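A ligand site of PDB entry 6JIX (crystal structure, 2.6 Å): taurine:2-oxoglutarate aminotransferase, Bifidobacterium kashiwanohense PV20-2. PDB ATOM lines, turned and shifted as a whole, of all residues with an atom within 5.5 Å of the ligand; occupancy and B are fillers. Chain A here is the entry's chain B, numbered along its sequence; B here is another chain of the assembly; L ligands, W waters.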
ATOM      1  N   GLY A 115      25.962 -22.136  27.376  1.00  0.00           N
ATOM      2  CA  GLY A 115      25.249 -23.341  26.980  1.00  0.00           C
ATOM      3  C   GLY A 115      25.802 -24.542  27.692  1.00  0.00           C
ATOM      4  O   GLY A 115      26.459 -24.417  28.721  1.00  0.00           O
ATOM      5  N   GLY A 116      25.575 -25.717  27.099  1.00  0.00           N
ATOM      6  CA  GLY A 116      26.041 -26.956  27.691  1.00  0.00           C
ATOM      7  C   GLY A 116      27.519 -27.256  27.501  1.00  0.00           C
ATOM      8  O   GLY A 116      28.210 -27.631  28.452  1.00  0.00           O
ATOM      9  N   ALA A 117      28.018 -27.102  26.271  1.00  0.00           N
ATOM     10  CA  ALA A 117      29.405 -27.462  25.995  1.00  0.00           C
ATOM     11  C   ALA A 117      30.377 -26.661  26.859  1.00  0.00           C
ATOM     12  O   ALA A 117      31.279 -27.241  27.468  1.00  0.00           O
ATOM     13  CB  ALA A 117      29.736 -27.290  24.512  1.00  0.00           C
ATOM     14  N   ASP A 118      30.197 -25.337  26.950  1.00  0.00           N
ATOM     15  CA  ASP A 118      31.190 -24.577  27.714  1.00  0.00           C
ATOM     16  C   ASP A 118      31.069 -24.857  29.206  1.00  0.00           C
ATOM     17  O   ASP A 118      32.061 -24.776  29.951  1.00  0.00           O
ATOM     18  CB  ASP A 118      31.202 -23.079  27.370  1.00  0.00           C
ATOM     19  CG  ASP A 118      29.841 -22.401  27.470  1.00  0.00           C
ATOM     20  OD1 ASP A 118      28.786 -23.059  27.575  1.00  0.00           O
ATOM     21  OD2 ASP A 118      29.847 -21.141  27.414  1.00  0.00           O
ATOM     22  N   ASN A 120      30.483 -27.873  30.476  1.00  0.00           N
ATOM     23  CA  ASN A 120      31.302 -29.060  30.693  1.00  0.00           C
ATOM     24  C   ASN A 120      32.792 -28.751  30.578  1.00  0.00           C
ATOM     25  O   ASN A 120      33.590 -29.262  31.364  1.00  0.00           O
ATOM     26  CB  ASN A 120      30.880 -30.172  29.726  1.00  0.00           C
ATOM     27  CG  ASN A 120      29.568 -30.806  30.156  1.00  0.00           C
ATOM     28  OD1 ASN A 120      29.281 -30.858  31.352  1.00  0.00           O
ATOM     29  ND2 ASN A 120      28.770 -31.253  29.207  1.00  0.00           N
ATOM     30  N   TYR A 143      27.169 -37.832  25.191  1.00  0.00           N
ATOM     31  CA  TYR A 143      27.468 -36.602  24.468  1.00  0.00           C
ATOM     32  C   TYR A 143      27.527 -35.437  25.450  1.00  0.00           C
ATOM     33  O   TYR A 143      26.622 -35.282  26.271  1.00  0.00           O
ATOM     34  CB  TYR A 143      26.423 -36.309  23.379  1.00  0.00           C
ATOM     35  CG  TYR A 143      26.729 -35.057  22.586  1.00  0.00           C
ATOM     36  CD1 TYR A 143      27.765 -35.026  21.658  1.00  0.00           C
ATOM     37  CD2 TYR A 143      25.978 -33.892  22.765  1.00  0.00           C
ATOM     38  CE1 TYR A 143      28.055 -33.872  20.921  1.00  0.00           C
ATOM     39  CE2 TYR A 143      26.246 -32.728  22.023  1.00  0.00           C
ATOM     40  CZ  TYR A 143      27.290 -32.727  21.101  1.00  0.00           C
ATOM     41  OH  TYR A 143      27.580 -31.573  20.364  1.00  0.00           O
ATOM     42  N   HIS A 144      28.596 -34.642  25.358  1.00  0.00           N
ATOM     43  CA  HIS A 144      28.821 -33.513  26.262  1.00  0.00           C
ATOM     44  C   HIS A 144      29.097 -32.189  25.562  1.00  0.00           C
ATOM     45  O   HIS A 144      29.429 -31.212  26.248  1.00  0.00           O
ATOM     46  CB  HIS A 144      29.992 -33.813  27.200  1.00  0.00           C
ATOM     47  CG  HIS A 144      29.756 -34.991  28.095  1.00  0.00           C
ATOM     48  ND1 HIS A 144      28.895 -34.954  29.160  1.00  0.00           N
ATOM     49  CD2 HIS A 144      30.269 -36.253  28.055  1.00  0.00           C
ATOM     50  CE1 HIS A 144      28.886 -36.138  29.762  1.00  0.00           C
ATOM     51  NE2 HIS A 144      29.721 -36.940  29.118  1.00  0.00           N
ATOM     52  N   GLY A 145      29.003 -32.129  24.242  1.00  0.00           N
ATOM     53  CA  GLY A 145      29.257 -30.903  23.508  1.00  0.00           C
ATOM     54  C   GLY A 145      30.249 -31.136  22.382  1.00  0.00           C
ATOM     55  O   GLY A 145      30.858 -32.194  22.255  1.00  0.00           O
ATOM     56  N   SER A 146      30.412 -30.087  21.568  1.00  0.00           N
ATOM     57  CA  SER A 146      31.168 -30.201  20.325  1.00  0.00           C
ATOM     58  C   SER A 146      32.474 -29.432  20.328  1.00  0.00           C
ATOM     59  O   SER A 146      33.314 -29.655  19.435  1.00  0.00           O
ATOM     60  CB  SER A 146      30.309 -29.735  19.141  1.00  0.00           C
ATOM     61  OG  SER A 146      29.580 -28.589  19.492  1.00  0.00           O
ATOM     62  N   GLU A 219      26.611 -38.089  32.012  1.00  0.00           N
ATOM     63  CA  GLU A 219      25.202 -37.721  31.968  1.00  0.00           C
ATOM     64  C   GLU A 219      24.436 -38.478  33.045  1.00  0.00           C
ATOM     65  O   GLU A 219      24.514 -39.709  33.131  1.00  0.00           O
ATOM     66  CB  GLU A 219      24.587 -38.045  30.607  1.00  0.00           C
ATOM     67  CG  GLU A 219      24.981 -37.166  29.453  1.00  0.00           C
ATOM     68  CD  GLU A 219      24.409 -37.672  28.126  1.00  0.00           C
ATOM     69  OE1 GLU A 219      23.314 -37.190  27.738  1.00  0.00           O
ATOM     70  OE2 GLU A 219      25.039 -38.527  27.471  1.00  0.00           O
ATOM     71  N   ALA A 224      20.696 -37.862  24.591  1.00  0.00           N
ATOM     72  CA  ALA A 224      20.516 -37.851  23.144  1.00  0.00           C
ATOM     73  C   ALA A 224      20.792 -39.217  22.554  1.00  0.00           C
ATOM     74  O   ALA A 224      20.141 -39.626  21.579  1.00  0.00           O
ATOM     75  CB  ALA A 224      21.386 -36.776  22.496  1.00  0.00           C
ATOM     76  N   ASP A 252      26.185 -34.479  34.198  1.00  0.00           N
ATOM     77  CA  ASP A 252      25.738 -33.582  33.126  1.00  0.00           C
ATOM     78  C   ASP A 252      24.207 -33.575  33.122  1.00  0.00           C
ATOM     79  O   ASP A 252      23.572 -34.557  32.746  1.00  0.00           O
ATOM     80  CB  ASP A 252      26.333 -34.045  31.796  1.00  0.00           C
ATOM     81  CG  ASP A 252      25.976 -33.137  30.630  1.00  0.00           C
ATOM     82  OD1 ASP A 252      24.920 -32.478  30.696  1.00  0.00           O
ATOM     83  OD2 ASP A 252      26.742 -33.109  29.633  1.00  0.00           O
ATOM     84  N   VAL A 254      22.525 -31.254  31.349  1.00  0.00           N
ATOM     85  CA  VAL A 254      22.154 -30.348  30.260  1.00  0.00           C
ATOM     86  C   VAL A 254      20.824 -30.772  29.640  1.00  0.00           C
ATOM     87  O   VAL A 254      19.952 -29.938  29.355  1.00  0.00           O
ATOM     88  CB  VAL A 254      23.283 -30.271  29.212  1.00  0.00           C
ATOM     89  CG1 VAL A 254      22.758 -29.721  27.884  1.00  0.00           C
ATOM     90  CG2 VAL A 254      24.432 -29.414  29.737  1.00  0.00           C
ATOM     91  N   MET A 255      20.651 -32.075  29.395  1.00  0.00           N
ATOM     92  CA  MET A 255      19.427 -32.564  28.782  1.00  0.00           C
ATOM     93  C   MET A 255      18.399 -33.062  29.797  1.00  0.00           C
ATOM     94  O   MET A 255      17.205 -32.870  29.598  1.00  0.00           O
ATOM     95  CB  MET A 255      19.733 -33.687  27.786  1.00  0.00           C
ATOM     96  CG  MET A 255      18.472 -34.333  27.226  1.00  0.00           C
ATOM     97  SD  MET A 255      18.676 -35.179  25.639  1.00  0.00           S
ATOM     98  CE  MET A 255      19.532 -33.899  24.724  1.00  0.00           C
ATOM     99  N   ALA A 280      22.169 -26.572  30.925  1.00  0.00           N
ATOM    100  CA  ALA A 280      21.836 -25.502  30.003  1.00  0.00           C
ATOM    101  C   ALA A 280      20.338 -25.438  29.741  1.00  0.00           C
ATOM    102  O   ALA A 280      19.634 -24.589  30.281  1.00  0.00           O
ATOM    103  CB  ALA A 280      22.580 -25.690  28.664  1.00  0.00           C
ATOM    104  N   LYS A 281      19.843 -26.413  28.992  1.00  0.00           N
ATOM    105  CA  LYS A 281      18.677 -26.195  28.151  1.00  0.00           C
ATOM    106  C   LYS A 281      17.503 -25.608  28.943  1.00  0.00           C
ATOM    107  O   LYS A 281      17.128 -24.448  28.733  1.00  0.00           O
ATOM    108  CB  LYS A 281      18.337 -27.527  27.482  1.00  0.00           C
ATOM    109  CG  LYS A 281      19.343 -27.863  26.411  1.00  0.00           C
ATOM    110  CD  LYS A 281      19.604 -29.335  26.358  1.00  0.00           C
ATOM    111  CE  LYS A 281      19.332 -29.795  24.964  1.00  0.00           C
ATOM    112  NZ  LYS A 281      20.298 -30.785  24.501  1.00  0.00           N
ATOM    113  N   ASN B 114      27.404 -19.157  20.092  1.00  0.00           N
ATOM    114  CA  ASN B 114      26.992 -18.409  21.276  1.00  0.00           C
ATOM    115  C   ASN B 114      27.926 -17.272  21.650  1.00  0.00           C
ATOM    116  O   ASN B 114      27.498 -16.341  22.331  1.00  0.00           O
ATOM    117  CB  ASN B 114      26.906 -19.345  22.490  1.00  0.00           C
ATOM    118  CG  ASN B 114      25.660 -20.194  22.511  1.00  0.00           C
ATOM    119  OD1 ASN B 114      24.614 -19.797  21.991  1.00  0.00           O
ATOM    120  ND2 ASN B 114      25.758 -21.383  23.110  1.00  0.00           N
ATOM    121  N   GLY B 311      28.146 -28.316  15.372  1.00  0.00           N
ATOM    122  CA  GLY B 311      26.791 -28.062  15.824  1.00  0.00           C
ATOM    123  C   GLY B 311      26.740 -27.604  17.268  1.00  0.00           C
ATOM    124  O   GLY B 311      27.704 -27.751  18.005  1.00  0.00           O
ATOM    125  N   LEU B 312      25.618 -27.005  17.657  1.00  0.00           N
ATOM    126  CA  LEU B 312      25.372 -26.691  19.050  1.00  0.00           C
ATOM    127  C   LEU B 312      23.894 -26.374  19.175  1.00  0.00           C
ATOM    128  O   LEU B 312      23.267 -25.915  18.210  1.00  0.00           O
ATOM    129  CB  LEU B 312      26.262 -25.524  19.538  1.00  0.00           C
ATOM    130  CG  LEU B 312      26.003 -24.166  18.897  1.00  0.00           C
ATOM    131  CD1 LEU B 312      26.092 -23.005  19.900  1.00  0.00           C
ATOM    132  CD2 LEU B 312      26.957 -23.968  17.747  1.00  0.00           C
ATOM    133  N   THR B 313      23.315 -26.686  20.338  1.00  0.00           N
ATOM    134  CA  THR B 313      21.871 -26.555  20.503  1.00  0.00           C
ATOM    135  C   THR B 313      21.391 -25.188  20.011  1.00  0.00           C
ATOM    136  O   THR B 313      20.442 -25.094  19.216  1.00  0.00           O
ATOM    137  CB  THR B 313      21.464 -26.787  21.963  1.00  0.00           C
ATOM    138  OG1 THR B 313      21.821 -28.120  22.339  1.00  0.00           O
ATOM    139  CG2 THR B 313      19.958 -26.597  22.160  1.00  0.00           C
ATOM    140  N   TYR B 314      22.071 -24.118  20.425  1.00  0.00           N
ATOM    141  CA  TYR B 314      21.586 -22.752  20.239  1.00  0.00           C
ATOM    142  C   TYR B 314      22.106 -22.075  18.971  1.00  0.00           C
ATOM    143  O   TYR B 314      21.999 -20.852  18.854  1.00  0.00           O
ATOM    144  CB  TYR B 314      21.932 -21.921  21.474  1.00  0.00           C
ATOM    145  CG  TYR B 314      21.176 -22.344  22.715  1.00  0.00           C
ATOM    146  CD1 TYR B 314      19.859 -22.835  22.627  1.00  0.00           C
ATOM    147  CD2 TYR B 314      21.766 -22.264  23.980  1.00  0.00           C
ATOM    148  CE1 TYR B 314      19.151 -23.237  23.780  1.00  0.00           C
ATOM    149  CE2 TYR B 314      21.078 -22.666  25.123  1.00  0.00           C
ATOM    150  CZ  TYR B 314      19.766 -23.144  25.016  1.00  0.00           C
ATOM    151  OH  TYR B 314      19.087 -23.517  26.156  1.00  0.00           O
HETATM  152  N1  LIG L   1      25.377 -32.375  27.391  1.00  0.00           N
HETATM  153  C1  LIG L   1      24.278 -33.039  27.016  1.00  0.00           C
HETATM  154  C2  LIG L   1      23.727 -34.164  27.880  1.00  0.00           C
HETATM  155  C3  LIG L   1      23.623 -32.710  25.808  1.00  0.00           C
HETATM  156  O1  LIG L   1      22.491 -33.384  25.395  1.00  0.00           O
HETATM  157  C4  LIG L   1      24.100 -31.693  25.020  1.00  0.00           C
HETATM  158  C5  LIG L   1      23.342 -31.365  23.698  1.00  0.00           C
HETATM  159  O2  LIG L   1      22.684 -32.225  23.114  1.00  0.00           O
HETATM  160  C6  LIG L   1      25.269 -31.006  25.458  1.00  0.00           C
HETATM  161  C7  LIG L   1      25.894 -31.366  26.656  1.00  0.00           C
HETATM  162  C8  LIG L   1      25.856 -29.837  24.584  1.00  0.00           C
HETATM  163  O3  LIG L   1      25.054 -28.730  24.855  1.00  0.00           O
HETATM  164  P1  LIG L   1      25.104 -27.435  23.877  1.00  0.00           P
HETATM  165  O4  LIG L   1      24.355 -26.318  24.469  1.00  0.00           O
HETATM  166  O5  LIG L   1      26.477 -26.893  23.757  1.00  0.00           O
HETATM  167  O6  LIG L   1      24.529 -27.877  22.364  1.00  0.00           O
HETATM  168  O   HOH W   1      26.727 -24.475  22.762  1.00  0.00           O
HETATM  169  O   HOH W   2      24.261 -24.241  22.656  1.00  0.00           O
HETATM  170  O   HOH W   3      21.890 -25.885  25.831  1.00  0.00           O
HETATM  171  O   HOH W   4      22.764 -34.451  20.667  1.00  0.00           O
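A nitrogen (N1) of the ligand lies close to the backbone carbonyl oxygen of Tyr 143.
Merely in contact with the ligand: Glu 219 (3.1 Å), Met 255 (3.1 Å), Val 254 (3.5 Å), His 144 (3.5 Å), Leu 312 of chain B (3.6 Å), Gly 145 (3.7 Å), Asn 120 (3.8 Å) and Gly 115 (3.95 Å).
Hydrophobic or aromatic side chains within 4 Å of the ligand: Ala 117, Tyr 143, Val 254 and Met 255.
Within 4 Å of the ligand: Gly 115, Gly 116, Ala 117, Asn 120, Tyr 143, His 144, Gly 145, Glu 219, Asp 252, Val 254, Met 255, Lys 281, Leu 312 of chain B and Thr 313 of chain B.
Water W1 lies within hydrogen-bond range of O5 of the ligand (2.6 Å) and ND2 of Asn 114 of chain B (3.3 Å).
An oxygen (O6) of the ligand is in hydrogen-bond range of the backbone NH (N) of Thr 313 of chain B, 2.6 Å away.
OG1 of Thr 313 of chain B lies within hydrogen-bond range of O6 of the ligand (2.7 Å).
OD2 of Asp 252 lies within hydrogen-bond range of N1 of the ligand (2.7 Å).
The backbone NH of Ala 117 is in hydrogen-bond range of an oxygen (O5) of the ligand.
N of Gly 116 is in hydrogen-bond range of O4 of the ligand, at 3.0 Å.
The side-chain amino group of Lys 281 sits at hydrogen-bond distance from an oxygen (O2) of the ligand, at 3.1 Å.
N of Val 254 sits at hydrogen-bond distance from OD1 of Asp 252, at 2.8 Å.
A ring nitrogen (ND1) of His 144 lies within hydrogen-bond range of the side-chain carboxylate (OD2) of Asp 252 (2.9 Å).
ND2 of Asn 120 is in hydrogen-bond range of OD2 of Asp 252, 2.8 Å away.
The side-chain sulfur of Met 255 lies within hydrogen-bond range of the backbone NH of Ala 224 (3.5 Å).
The side-chain hydroxyl of Tyr 314 of chain B sits close to the backbone carbonyl oxygen of Lys 281 (3.4 Å).
The side-chain hydroxyl of Tyr 143 sits at hydrogen-bond distance from the backbone NH of Ser 146 (3.4 Å).
O of His 144 lies within hydrogen-bond range of ND2 of Asn 120 (3.0 Å).
The backbone NH (N) of Gly 115 lies within hydrogen-bond range of the side-chain carboxylate (OD1) of Asp 118.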
